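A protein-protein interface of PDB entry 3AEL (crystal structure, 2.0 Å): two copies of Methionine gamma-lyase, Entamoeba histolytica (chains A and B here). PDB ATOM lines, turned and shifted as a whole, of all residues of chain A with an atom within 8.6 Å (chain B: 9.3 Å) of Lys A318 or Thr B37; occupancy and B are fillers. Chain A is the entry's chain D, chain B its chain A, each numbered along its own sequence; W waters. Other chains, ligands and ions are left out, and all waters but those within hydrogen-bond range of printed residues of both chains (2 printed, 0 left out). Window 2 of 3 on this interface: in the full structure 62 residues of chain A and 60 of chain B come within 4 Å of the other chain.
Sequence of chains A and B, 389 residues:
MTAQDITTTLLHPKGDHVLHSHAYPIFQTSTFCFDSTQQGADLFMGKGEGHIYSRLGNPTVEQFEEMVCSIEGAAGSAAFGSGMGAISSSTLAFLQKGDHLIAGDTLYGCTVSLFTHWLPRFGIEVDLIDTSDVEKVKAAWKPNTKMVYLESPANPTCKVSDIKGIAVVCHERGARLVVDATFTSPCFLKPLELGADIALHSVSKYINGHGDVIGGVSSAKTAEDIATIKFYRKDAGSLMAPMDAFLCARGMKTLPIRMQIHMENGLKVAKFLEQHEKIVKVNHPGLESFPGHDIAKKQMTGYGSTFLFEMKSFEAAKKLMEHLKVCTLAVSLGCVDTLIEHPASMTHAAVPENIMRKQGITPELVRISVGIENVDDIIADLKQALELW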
ATOM      1  N   MET A 311       3.621  25.876 -14.555  1.00  0.00           N
ATOM      2  CA  MET A 311       3.395  27.312 -14.814  1.00  0.00           C
ATOM      3  C   MET A 311       2.432  27.453 -15.987  1.00  0.00           C
ATOM      4  O   MET A 311       2.073  26.453 -16.606  1.00  0.00           O
ATOM      5  CB  MET A 311       4.700  28.044 -15.149  1.00  0.00           C
ATOM      6  CG  MET A 311       5.784  28.011 -14.080  1.00  0.00           C
ATOM      7  SD  MET A 311       5.281  28.728 -12.512  1.00  0.00           S
ATOM      8  CE  MET A 311       4.896  30.441 -12.897  1.00  0.00           C
ATOM      9  N   SER A 313       3.146  29.165 -18.764  1.00  0.00           N
ATOM     10  CA  SER A 313       3.906  29.115 -20.015  1.00  0.00           C
ATOM     11  C   SER A 313       5.384  28.860 -19.734  1.00  0.00           C
ATOM     12  O   SER A 313       5.802  28.878 -18.574  1.00  0.00           O
ATOM     13  CB  SER A 313       3.728  30.410 -20.818  1.00  0.00           C
ATOM     14  OG  SER A 313       4.500  31.442 -20.242  1.00  0.00           O
ATOM     15  N   PHE A 314       6.177  28.636 -20.784  1.00  0.00           N
ATOM     16  CA  PHE A 314       7.626  28.590 -20.596  1.00  0.00           C
ATOM     17  C   PHE A 314       8.177  29.932 -20.087  1.00  0.00           C
ATOM     18  O   PHE A 314       9.010  29.941 -19.182  1.00  0.00           O
ATOM     19  CB  PHE A 314       8.375  28.135 -21.854  1.00  0.00           C
ATOM     20  CG  PHE A 314       9.870  28.286 -21.743  1.00  0.00           C
ATOM     21  CD1 PHE A 314      10.551  29.231 -22.510  1.00  0.00           C
ATOM     22  CD2 PHE A 314      10.596  27.512 -20.842  1.00  0.00           C
ATOM     23  CE1 PHE A 314      11.948  29.392 -22.384  1.00  0.00           C
ATOM     24  CE2 PHE A 314      11.988  27.663 -20.719  1.00  0.00           C
ATOM     25  CZ  PHE A 314      12.656  28.610 -21.487  1.00  0.00           C
ATOM     26  N   GLU A 315       7.707  31.049 -20.660  1.00  0.00           N
ATOM     27  CA  GLU A 315       8.195  32.391 -20.290  1.00  0.00           C
ATOM     28  C   GLU A 315       7.986  32.693 -18.808  1.00  0.00           C
ATOM     29  O   GLU A 315       8.839  33.308 -18.165  1.00  0.00           O
ATOM     30  CB  GLU A 315       7.543  33.502 -21.144  1.00  0.00           C
ATOM     31  CG  GLU A 315       7.978  33.521 -22.634  1.00  0.00           C
ATOM     32  CD  GLU A 315       9.490  33.329 -22.845  1.00  0.00           C
ATOM     33  OE1 GLU A 315       9.878  32.483 -23.699  1.00  0.00           O
ATOM     34  OE2 GLU A 315      10.294  34.011 -22.154  1.00  0.00           O
ATOM     35  N   ALA A 316       6.838  32.260 -18.289  1.00  0.00           N
ATOM     36  CA  ALA A 316       6.484  32.396 -16.884  1.00  0.00           C
ATOM     37  C   ALA A 316       7.401  31.546 -15.987  1.00  0.00           C
ATOM     38  O   ALA A 316       7.806  31.984 -14.905  1.00  0.00           O
ATOM     39  CB  ALA A 316       5.027  32.021 -16.676  1.00  0.00           C
ATOM     40  N   ALA A 317       7.708  30.328 -16.424  1.00  0.00           N
ATOM     41  CA  ALA A 317       8.620  29.479 -15.664  1.00  0.00           C
ATOM     42  C   ALA A 317      10.015  30.097 -15.620  1.00  0.00           C
ATOM     43  O   ALA A 317      10.653  30.130 -14.575  1.00  0.00           O
ATOM     44  CB  ALA A 317       8.660  28.086 -16.245  1.00  0.00           C
ATOM     45  N   LYS A 318      10.464  30.614 -16.761  1.00  0.00           N
ATOM     46  CA  LYS A 318      11.775  31.248 -16.880  1.00  0.00           C
ATOM     47  C   LYS A 318      11.841  32.472 -15.974  1.00  0.00           C
ATOM     48  O   LYS A 318      12.822  32.682 -15.266  1.00  0.00           O
ATOM     49  CB  LYS A 318      12.050  31.636 -18.338  1.00  0.00           C
ATOM     50  CG  LYS A 318      13.380  32.349 -18.568  1.00  0.00           C
ATOM     51  CD  LYS A 318      13.418  32.995 -19.960  1.00  0.00           C
ATOM     52  CE  LYS A 318      14.476  34.097 -20.049  1.00  0.00           C
ATOM     53  NZ  LYS A 318      14.560  34.651 -21.432  1.00  0.00           N
ATOM     54  N   LYS A 319      10.787  33.274 -15.991  1.00  0.00           N
ATOM     55  CA  LYS A 319      10.746  34.439 -15.130  1.00  0.00           C
ATOM     56  C   LYS A 319      10.815  34.051 -13.647  1.00  0.00           C
ATOM     57  O   LYS A 319      11.552  34.672 -12.872  1.00  0.00           O
ATOM     58  CB  LYS A 319       9.521  35.312 -15.424  1.00  0.00           C
ATOM     59  CG  LYS A 319       9.851  36.789 -15.336  1.00  0.00           C
ATOM     60  CD  LYS A 319       8.630  37.675 -15.401  1.00  0.00           C
ATOM     61  CE  LYS A 319       8.912  38.999 -14.692  1.00  0.00           C
ATOM     62  NZ  LYS A 319       7.664  39.798 -14.564  1.00  0.00           N
ATOM     63  N   LEU A 320      10.072  33.017 -13.256  1.00  0.00           N
ATOM     64  CA  LEU A 320      10.102  32.578 -11.872  1.00  0.00           C
ATOM     65  C   LEU A 320      11.489  32.062 -11.476  1.00  0.00           C
ATOM     66  O   LEU A 320      12.046  32.494 -10.467  1.00  0.00           O
ATOM     67  CB  LEU A 320       9.039  31.513 -11.597  1.00  0.00           C
ATOM     68  CG  LEU A 320       9.256  30.729 -10.294  1.00  0.00           C
ATOM     69  CD1 LEU A 320       9.071  31.603  -9.031  1.00  0.00           C
ATOM     70  CD2 LEU A 320       8.331  29.521 -10.284  1.00  0.00           C
ATOM     71  N   MET A 321      12.043  31.160 -12.280  1.00  0.00           N
ATOM     72  CA  MET A 321      13.334  30.528 -11.969  1.00  0.00           C
ATOM     73  C   MET A 321      14.512  31.490 -11.997  1.00  0.00           C
ATOM     74  O   MET A 321      15.578  31.183 -11.449  1.00  0.00           O
ATOM     75  CB  MET A 321      13.634  29.392 -12.944  1.00  0.00           C
ATOM     76  CG  MET A 321      12.796  28.153 -12.750  1.00  0.00           C
ATOM     77  SD  MET A 321      13.253  26.898 -13.961  1.00  0.00           S
ATOM     78  CE  MET A 321      12.698  27.646 -15.486  1.00  0.00           C
ATOM     79  N   GLU A 322      14.339  32.631 -12.650  1.00  0.00           N
ATOM     80  CA  GLU A 322      15.447  33.561 -12.834  1.00  0.00           C
ATOM     81  C   GLU A 322      15.398  34.792 -11.918  1.00  0.00           C
ATOM     82  O   GLU A 322      16.282  35.651 -12.003  1.00  0.00           O
ATOM     83  CB  GLU A 322      15.552  33.988 -14.303  1.00  0.00           C
ATOM     84  CG  GLU A 322      16.135  32.916 -15.200  1.00  0.00           C
ATOM     85  CD  GLU A 322      16.172  33.314 -16.667  1.00  0.00           C
ATOM     86  OE1 GLU A 322      16.522  32.452 -17.503  1.00  0.00           O
ATOM     87  OE2 GLU A 322      15.844  34.476 -17.000  1.00  0.00           O
ATOM     88  N   HIS A 323      14.395  34.868 -11.037  1.00  0.00           N
ATOM     89  CA  HIS A 323      14.269  35.996 -10.074  1.00  0.00           C
ATOM     90  C   HIS A 323      14.182  35.599  -8.598  1.00  0.00           C
ATOM     91  O   HIS A 323      13.676  36.354  -7.773  1.00  0.00           O
ATOM     92  CB  HIS A 323      13.106  36.913 -10.462  1.00  0.00           C
ATOM     93  CG  HIS A 323      13.326  37.601 -11.768  1.00  0.00           C
ATOM     94  ND1 HIS A 323      12.990  37.024 -12.974  1.00  0.00           N
ATOM     95  CD2 HIS A 323      13.914  38.781 -12.062  1.00  0.00           C
ATOM     96  CE1 HIS A 323      13.328  37.839 -13.956  1.00  0.00           C
ATOM     97  NE2 HIS A 323      13.885  38.915 -13.430  1.00  0.00           N
ATOM     98  N   LEU A 324      14.694  34.420  -8.276  1.00  0.00           N
ATOM     99  CA  LEU A 324      14.736  33.939  -6.902  1.00  0.00           C
ATOM    100  C   LEU A 324      16.050  34.355  -6.280  1.00  0.00           C
ATOM    101  O   LEU A 324      17.088  34.266  -6.918  1.00  0.00           O
ATOM    102  CB  LEU A 324      14.596  32.417  -6.874  1.00  0.00           C
ATOM    103  CG  LEU A 324      13.258  31.924  -7.427  1.00  0.00           C
ATOM    104  CD1 LEU A 324      13.404  30.506  -7.944  1.00  0.00           C
ATOM    105  CD2 LEU A 324      12.131  32.042  -6.393  1.00  0.00           C
ATOM    106  N   LEU A 329      19.217  28.153  -8.662  1.00  0.00           N
ATOM    107  CA  LEU A 329      18.993  27.462  -9.908  1.00  0.00           C
ATOM    108  C   LEU A 329      20.144  26.453 -10.135  1.00  0.00           C
ATOM    109  O   LEU A 329      21.283  26.830 -10.424  1.00  0.00           O
ATOM    110  CB  LEU A 329      18.874  28.477 -11.050  1.00  0.00           C
ATOM    111  CG  LEU A 329      18.511  27.929 -12.442  1.00  0.00           C
ATOM    112  CD1 LEU A 329      17.132  27.244 -12.430  1.00  0.00           C
ATOM    113  CD2 LEU A 329      18.571  29.037 -13.516  1.00  0.00           C
ATOM    114  N   ILE A 340      16.115  24.664  -7.425  1.00  0.00           N
ATOM    115  CA  ILE A 340      15.048  24.705  -8.384  1.00  0.00           C
ATOM    116  C   ILE A 340      15.615  24.422  -9.784  1.00  0.00           C
ATOM    117  O   ILE A 340      16.727  24.866 -10.120  1.00  0.00           O
ATOM    118  CB  ILE A 340      14.290  26.063  -8.267  1.00  0.00           C
ATOM    119  CG1 ILE A 340      12.919  25.985  -8.928  1.00  0.00           C
ATOM    120  CG2 ILE A 340      15.141  27.199  -8.837  1.00  0.00           C
ATOM    121  CD1 ILE A 340      11.889  27.070  -8.400  1.00  0.00           C
ATOM    122  N   GLU A 341      14.878  23.649 -10.585  1.00  0.00           N
ATOM    123  CA  GLU A 341      15.319  23.328 -11.946  1.00  0.00           C
ATOM    124  C   GLU A 341      14.185  23.168 -12.968  1.00  0.00           C
ATOM    125  O   GLU A 341      13.010  23.081 -12.615  1.00  0.00           O
ATOM    126  CB  GLU A 341      16.251  22.092 -11.971  1.00  0.00           C
ATOM    127  CG  GLU A 341      15.575  20.775 -11.628  1.00  0.00           C
ATOM    128  CD  GLU A 341      15.458  19.816 -12.821  1.00  0.00           C
ATOM    129  OE1 GLU A 341      14.801  18.765 -12.689  1.00  0.00           O
ATOM    130  OE2 GLU A 341      16.030  20.098 -13.894  1.00  0.00           O
ATOM    131  N   HIS A 342      14.581  23.094 -14.241  1.00  0.00           N
ATOM    132  CA  HIS A 342      13.650  22.968 -15.371  1.00  0.00           C
ATOM    133  C   HIS A 342      13.897  21.622 -16.032  1.00  0.00           C
ATOM    134  O   HIS A 342      14.781  21.506 -16.879  1.00  0.00           O
ATOM    135  CB  HIS A 342      13.871  24.107 -16.364  1.00  0.00           C
ATOM    136  CG  HIS A 342      12.881  24.141 -17.487  1.00  0.00           C
ATOM    137  ND1 HIS A 342      13.235  23.898 -18.798  1.00  0.00           N
ATOM    138  CD2 HIS A 342      11.551  24.410 -17.497  1.00  0.00           C
ATOM    139  CE1 HIS A 342      12.167  24.017 -19.567  1.00  0.00           C
ATOM    140  NE2 HIS A 342      11.131  24.315 -18.801  1.00  0.00           N
ATOM    141  N   SER A 345      14.584  20.886 -20.001  1.00  0.00           N
ATOM    142  CA  SER A 345      15.853  21.319 -20.637  1.00  0.00           C
ATOM    143  C   SER A 345      17.092  21.002 -19.791  1.00  0.00           C
ATOM    144  O   SER A 345      18.223  21.324 -20.181  1.00  0.00           O
ATOM    145  CB  SER A 345      15.815  22.810 -21.023  1.00  0.00           C
ATOM    146  OG  SER A 345      15.819  23.640 -19.866  1.00  0.00           O
ATOM    147  N   MET A 346      16.879  20.336 -18.658  1.00  0.00           N
ATOM    148  CA  MET A 346      17.961  19.998 -17.733  1.00  0.00           C
ATOM    149  C   MET A 346      17.989  18.484 -17.383  1.00  0.00           C
ATOM    150  O   MET A 346      18.470  17.676 -18.195  1.00  0.00           O
ATOM    151  CB  MET A 346      17.928  20.918 -16.491  1.00  0.00           C
ATOM    152  CG  MET A 346      17.967  22.429 -16.829  1.00  0.00           C
ATOM    153  SD  MET A 346      17.948  23.504 -15.364  1.00  0.00           S
ATOM    154  CE  MET A 346      17.620  25.125 -16.050  1.00  0.00           C
ATOM    155  N   PRO A 363       7.588  21.975 -21.252  1.00  0.00           N
ATOM    156  CA  PRO A 363       8.398  23.141 -20.870  1.00  0.00           C
ATOM    157  C   PRO A 363       7.745  24.057 -19.807  1.00  0.00           C
ATOM    158  O   PRO A 363       8.397  24.990 -19.324  1.00  0.00           O
ATOM    159  CB  PRO A 363       8.575  23.904 -22.194  1.00  0.00           C
ATOM    160  CG  PRO A 363       7.937  23.032 -23.275  1.00  0.00           C
ATOM    161  CD  PRO A 363       6.994  22.118 -22.593  1.00  0.00           C
ATOM    162  N   GLU A 364       6.489  23.788 -19.446  1.00  0.00           N
ATOM    163  CA  GLU A 364       5.787  24.572 -18.406  1.00  0.00           C
ATOM    164  C   GLU A 364       6.112  24.128 -16.973  1.00  0.00           C
ATOM    165  O   GLU A 364       5.738  24.812 -16.017  1.00  0.00           O
ATOM    166  CB  GLU A 364       4.259  24.539 -18.612  1.00  0.00           C
ATOM    167  CG  GLU A 364       3.741  25.283 -19.835  1.00  0.00           C
ATOM    168  CD  GLU A 364       4.031  24.563 -21.144  1.00  0.00           C
ATOM    169  OE1 GLU A 364       3.996  25.229 -22.194  1.00  0.00           O
ATOM    170  OE2 GLU A 364       4.303  23.341 -21.144  1.00  0.00           O
ATOM    171  N   LEU A 365       6.795  22.992 -16.820  1.00  0.00           N
ATOM    172  CA  LEU A 365       7.076  22.422 -15.482  1.00  0.00           C
ATOM    173  C   LEU A 365       8.373  22.923 -14.865  1.00  0.00           C
ATOM    174  O   LEU A 365       9.398  23.017 -15.544  1.00  0.00           O
ATOM    175  CB  LEU A 365       7.060  20.886 -15.516  1.00  0.00           C
ATOM    176  CG  LEU A 365       5.844  20.261 -16.216  1.00  0.00           C
ATOM    177  CD1 LEU A 365       5.956  18.773 -16.262  1.00  0.00           C
ATOM    178  CD2 LEU A 365       4.543  20.639 -15.532  1.00  0.00           C
ATOM    179  N   VAL A 366       8.293  23.265 -13.574  1.00  0.00           N
ATOM    180  CA  VAL A 366       9.446  23.611 -12.733  1.00  0.00           C
ATOM    181  C   VAL A 366       9.545  22.590 -11.588  1.00  0.00           C
ATOM    182  O   VAL A 366       8.525  22.243 -10.994  1.00  0.00           O
ATOM    183  CB  VAL A 366       9.290  25.036 -12.145  1.00  0.00           C
ATOM    184  CG1 VAL A 366      10.411  25.376 -11.155  1.00  0.00           C
ATOM    185  CG2 VAL A 366       9.244  26.054 -13.277  1.00  0.00           C
ATOM    186  N   ALA A 385       9.105  36.488  -6.522  1.00  0.00           N
ATOM    187  CA  ALA A 385       9.461  35.996  -7.868  1.00  0.00           C
ATOM    188  C   ALA A 385       8.252  35.655  -8.750  1.00  0.00           C
ATOM    189  O   ALA A 385       8.398  35.500  -9.955  1.00  0.00           O
ATOM    190  CB  ALA A 385      10.348  34.802  -7.758  1.00  0.00           C
ATOM    191  N   CYS B  33      25.919  25.941  -9.886  1.00  0.00           N
ATOM    192  CA  CYS B  33      24.840  26.912 -10.087  1.00  0.00           C
ATOM    193  C   CYS B  33      24.787  27.411 -11.521  1.00  0.00           C
ATOM    194  O   CYS B  33      25.837  27.540 -12.192  1.00  0.00           O
ATOM    195  CB  CYS B  33      24.968  28.098  -9.101  1.00  0.00           C
ATOM    196  SG  CYS B  33      25.287  27.558  -7.417  1.00  0.00           S
ATOM    197  N   PHE B  34      23.569  27.702 -11.983  1.00  0.00           N
ATOM    198  CA  PHE B  34      23.366  28.270 -13.303  1.00  0.00           C
ATOM    199  C   PHE B  34      23.081  29.759 -13.182  1.00  0.00           C
ATOM    200  O   PHE B  34      22.379  30.190 -12.254  1.00  0.00           O
ATOM    201  CB  PHE B  34      22.197  27.584 -14.031  1.00  0.00           C
ATOM    202  CG  PHE B  34      22.398  26.101 -14.309  1.00  0.00           C
ATOM    203  CD1 PHE B  34      23.657  25.578 -14.653  1.00  0.00           C
ATOM    204  CD2 PHE B  34      21.306  25.233 -14.283  1.00  0.00           C
ATOM    205  CE1 PHE B  34      23.818  24.195 -14.938  1.00  0.00           C
ATOM    206  CE2 PHE B  34      21.456  23.873 -14.586  1.00  0.00           C
ATOM    207  CZ  PHE B  34      22.735  23.350 -14.914  1.00  0.00           C
ATOM    208  N   ASP B  35      23.610  30.549 -14.115  1.00  0.00           N
ATOM    209  CA  ASP B  35      23.280  31.987 -14.184  1.00  0.00           C
ATOM    210  C   ASP B  35      21.844  32.253 -14.634  1.00  0.00           C
ATOM    211  O   ASP B  35      21.269  33.300 -14.310  1.00  0.00           O
ATOM    212  CB  ASP B  35      24.197  32.727 -15.176  1.00  0.00           C
ATOM    213  CG  ASP B  35      25.675  32.584 -14.848  1.00  0.00           C
ATOM    214  OD1 ASP B  35      26.053  32.625 -13.650  1.00  0.00           O
ATOM    215  OD2 ASP B  35      26.458  32.455 -15.817  1.00  0.00           O
ATOM    216  N   SER B  36      21.293  31.333 -15.426  1.00  0.00           N
ATOM    217  CA  SER B  36      20.023  31.559 -16.120  1.00  0.00           C
ATOM    218  C   SER B  36      19.546  30.213 -16.620  1.00  0.00           C
ATOM    219  O   SER B  36      20.333  29.240 -16.657  1.00  0.00           O
ATOM    220  CB  SER B  36      20.218  32.497 -17.319  1.00  0.00           C
ATOM    221  OG  SER B  36      20.867  31.819 -18.394  1.00  0.00           O
ATOM    222  N   THR B  37      18.281  30.129 -17.027  1.00  0.00           N
ATOM    223  CA  THR B  37      17.824  28.833 -17.530  1.00  0.00           C
ATOM    224  C   THR B  37      18.529  28.480 -18.866  1.00  0.00           C
ATOM    225  O   THR B  37      18.875  27.313 -19.099  1.00  0.00           O
ATOM    226  CB  THR B  37      16.249  28.653 -17.562  1.00  0.00           C
ATOM    227  OG1 THR B  37      15.768  28.590 -18.904  1.00  0.00           O
ATOM    228  CG2 THR B  37      15.523  29.732 -16.810  1.00  0.00           C
ATOM    229  N   GLN B  38      18.776  29.497 -19.700  1.00  0.00           N
ATOM    230  CA  GLN B  38      19.470  29.338 -20.982  1.00  0.00           C
ATOM    231  C   GLN B  38      20.916  28.853 -20.815  1.00  0.00           C
ATOM    232  O   GLN B  38      21.376  27.920 -21.517  1.00  0.00           O
ATOM    233  CB  GLN B  38      19.449  30.646 -21.786  1.00  0.00           C
ATOM    234  CG  GLN B  38      19.812  30.439 -23.267  1.00  0.00           C
ATOM    235  CD  GLN B  38      18.912  29.399 -23.939  1.00  0.00           C
ATOM    236  OE1 GLN B  38      17.704  29.608 -24.097  1.00  0.00           O
ATOM    237  NE2 GLN B  38      19.499  28.272 -24.332  1.00  0.00           N
ATOM    238  N   GLN B  39      21.634  29.478 -19.885  1.00  0.00           N
ATOM    239  CA  GLN B  39      23.004  29.069 -19.622  1.00  0.00           C
ATOM    240  C   GLN B  39      23.059  27.603 -19.193  1.00  0.00           C
ATOM    241  O   GLN B  39      23.918  26.866 -19.657  1.00  0.00           O
ATOM    242  CB  GLN B  39      23.683  30.001 -18.615  1.00  0.00           C
ATOM    243  CG  GLN B  39      25.180  29.689 -18.414  1.00  0.00           C
ATOM    244  CD  GLN B  39      25.440  28.954 -17.109  1.00  0.00           C
ATOM    245  OE1 GLN B  39      24.574  28.900 -16.224  1.00  0.00           O
ATOM    246  NE2 GLN B  39      26.643  28.405 -16.968  1.00  0.00           N
ATOM    247  N   GLY B  40      22.117  27.180 -18.338  1.00  0.00           N
ATOM    248  CA  GLY B  40      22.013  25.768 -17.911  1.00  0.00           C
ATOM    249  C   GLY B  40      21.607  24.841 -19.053  1.00  0.00           C
ATOM    250  O   GLY B  40      22.202  23.761 -19.253  1.00  0.00           O
ATOM    251  N   ALA B  41      20.600  25.269 -19.811  1.00  0.00           N
ATOM    252  CA  ALA B  41      20.088  24.481 -20.915  1.00  0.00           C
ATOM    253  C   ALA B  41      21.200  24.197 -21.916  1.00  0.00           C
ATOM    254  O   ALA B  41      21.352  23.063 -22.372  1.00  0.00           O
ATOM    255  CB  ALA B  41      18.888  25.186 -21.607  1.00  0.00           C
ATOM    256  N   ASP B  42      21.965  25.245 -22.235  1.00  0.00           N
ATOM    257  CA  ASP B  42      23.109  25.185 -23.143  1.00  0.00           C
ATOM    258  C   ASP B  42      24.183  24.202 -22.670  1.00  0.00           C
ATOM    259  O   ASP B  42      24.679  23.389 -23.468  1.00  0.00           O
ATOM    260  CB  ASP B  42      23.715  26.576 -23.316  1.00  0.00           C
ATOM    261  CG  ASP B  42      22.888  27.473 -24.236  1.00  0.00           C
ATOM    262  OD1 ASP B  42      21.855  27.043 -24.794  1.00  0.00           O
ATOM    263  OD2 ASP B  42      23.284  28.632 -24.421  1.00  0.00           O
ATOM    264  N   LEU B  43      24.529  24.258 -21.380  1.00  0.00           N
ATOM    265  CA  LEU B  43      25.556  23.355 -20.849  1.00  0.00           C
ATOM    266  C   LEU B  43      25.100  21.920 -21.054  1.00  0.00           C
ATOM    267  O   LEU B  43      25.896  21.069 -21.414  1.00  0.00           O
ATOM    268  CB  LEU B  43      25.874  23.621 -19.363  1.00  0.00           C
ATOM    269  CG  LEU B  43      26.701  24.877 -19.072  1.00  0.00           C
ATOM    270  CD1 LEU B  43      26.941  25.082 -17.559  1.00  0.00           C
ATOM    271  CD2 LEU B  43      28.048  24.857 -19.827  1.00  0.00           C
ATOM    272  N   PHE B  44      23.803  21.660 -20.864  1.00  0.00           N
ATOM    273  CA  PHE B  44      23.273  20.316 -21.100  1.00  0.00           C
ATOM    274  C   PHE B  44      23.353  19.865 -22.564  1.00  0.00           C
ATOM    275  O   PHE B  44      23.426  18.654 -22.836  1.00  0.00           O
ATOM    276  CB  PHE B  44      21.857  20.181 -20.582  1.00  0.00           C
ATOM    277  CG  PHE B  44      21.776  19.701 -19.163  1.00  0.00           C
ATOM    278  CD1 PHE B  44      21.589  20.595 -18.128  1.00  0.00           C
ATOM    279  CD2 PHE B  44      21.877  18.341 -18.873  1.00  0.00           C
ATOM    280  CE1 PHE B  44      21.510  20.145 -16.808  1.00  0.00           C
ATOM    281  CE2 PHE B  44      21.786  17.878 -17.563  1.00  0.00           C
ATOM    282  CZ  PHE B  44      21.597  18.779 -16.528  1.00  0.00           C
ATOM    283  N   MET B  45      23.352  20.838 -23.478  1.00  0.00           N
ATOM    284  CA  MET B  45      23.527  20.596 -24.913  1.00  0.00           C
ATOM    285  C   MET B  45      24.992  20.571 -25.329  1.00  0.00           C
ATOM    286  O   MET B  45      25.301  20.410 -26.504  1.00  0.00           O
ATOM    287  CB  MET B  45      22.790  21.659 -25.722  1.00  0.00           C
ATOM    288  CG  MET B  45      21.273  21.548 -25.643  1.00  0.00           C
ATOM    289  SD  MET B  45      20.479  22.786 -26.705  1.00  0.00           S
ATOM    290  CE  MET B  45      20.203  24.224 -25.644  1.00  0.00           C
HETATM  291  O   HOH W   1      17.664  32.268 -19.880  1.00  0.00           O
HETATM  292  O   HOH W   2      19.070  21.305 -22.589  1.00  0.00           O
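The backbone NH (N) of Phe B34 sits at hydrogen-bond distance from the backbone carbonyl oxygen (O) of Leu A329 (2.9 Å). The backbone NH (N) of Thr B37 sits at hydrogen-bond distance from the side-chain carboxylate (OE1) of Glu A322, at 3.0 Å.
The side-chain hydroxyl (OG) of Ser B36 lies close to the backbone NH (N) of Gln B38 (3.4 Å). N of Gln B39 is in hydrogen-bond range of OG of Ser B36, 2.9 Å away. The side-chain hydroxyl (OG) of Ser A345 is in hydrogen-bond range of a ring nitrogen (ND1) of His A342. The backbone NH (N) of His A342 sits at hydrogen-bond distance from the side-chain sulfur (SD) of Met A346.
Among the printed residues, merely in contact across the chains: Lys A318 with Thr B37, Met A321 with Thr B37, Glu A322 with Ser B36, Leu A329 with Cys B33, Leu A329 with Ser B36, Leu A329 with Thr B37, Ser A345 with Ala B41, Ser A345 with Phe B44, Met A346 with Phe B34, Met A346 with Thr B37 and Met A346 with Phe B44.
Of chain B, only Thr B37 (3.8 Å) comes within 4 Å of Lys A318. Of chain A, only Lys A318, Met A321, Glu A322, Leu A329 and Met A346 come within 4 Å of Thr B37. No residue of chain B comes within 4 Å of Ala A317. Met A321 touches just one residue of chain B: Thr B37. Of the printed residues of chain A, Ser B36 touches Glu A322 and Leu A329. Of the printed residues of chain A, Phe B34 touches Leu A329 (2.9 Å) and Met A346 (3.6 Å). Printed residues of chain B within 4 Å of Ser A345: Ala B41 and Phe B44. Of the printed residues of chain B, Glu A322 touches Ser B36 (3.7 Å) and Thr B37 (3.0 Å). Met A311 touches none of the printed residues of chain B. The nearest residue of chain B that does not touch Lys A318 is Gln B38 (6.2 Å). The nearest residue of chain A that does not touch Thr B37 is Phe A314 (4.04 Å).
Of the 13 printed residues of chain B, 6 touch a printed residue of chain A. Hydrophobic or aromatic side chains of chain B that line the printed part of chain A: Phe B34, Ala B41 and Phe B44. Of the 24 printed residues of chain A, 6 touch a printed residue of chain B. Among the printed residues, 13 pairs touch across the chains.
No position is printed for both chains.
Water W2 lies within hydrogen-bond range of O of Ser A345 and O of Ala B41. Water W1 lies within hydrogen-bond range of the side-chain carboxylate of Glu A322 (2.6 Å) and the backbone NH of Gln B38 (3.0 Å).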
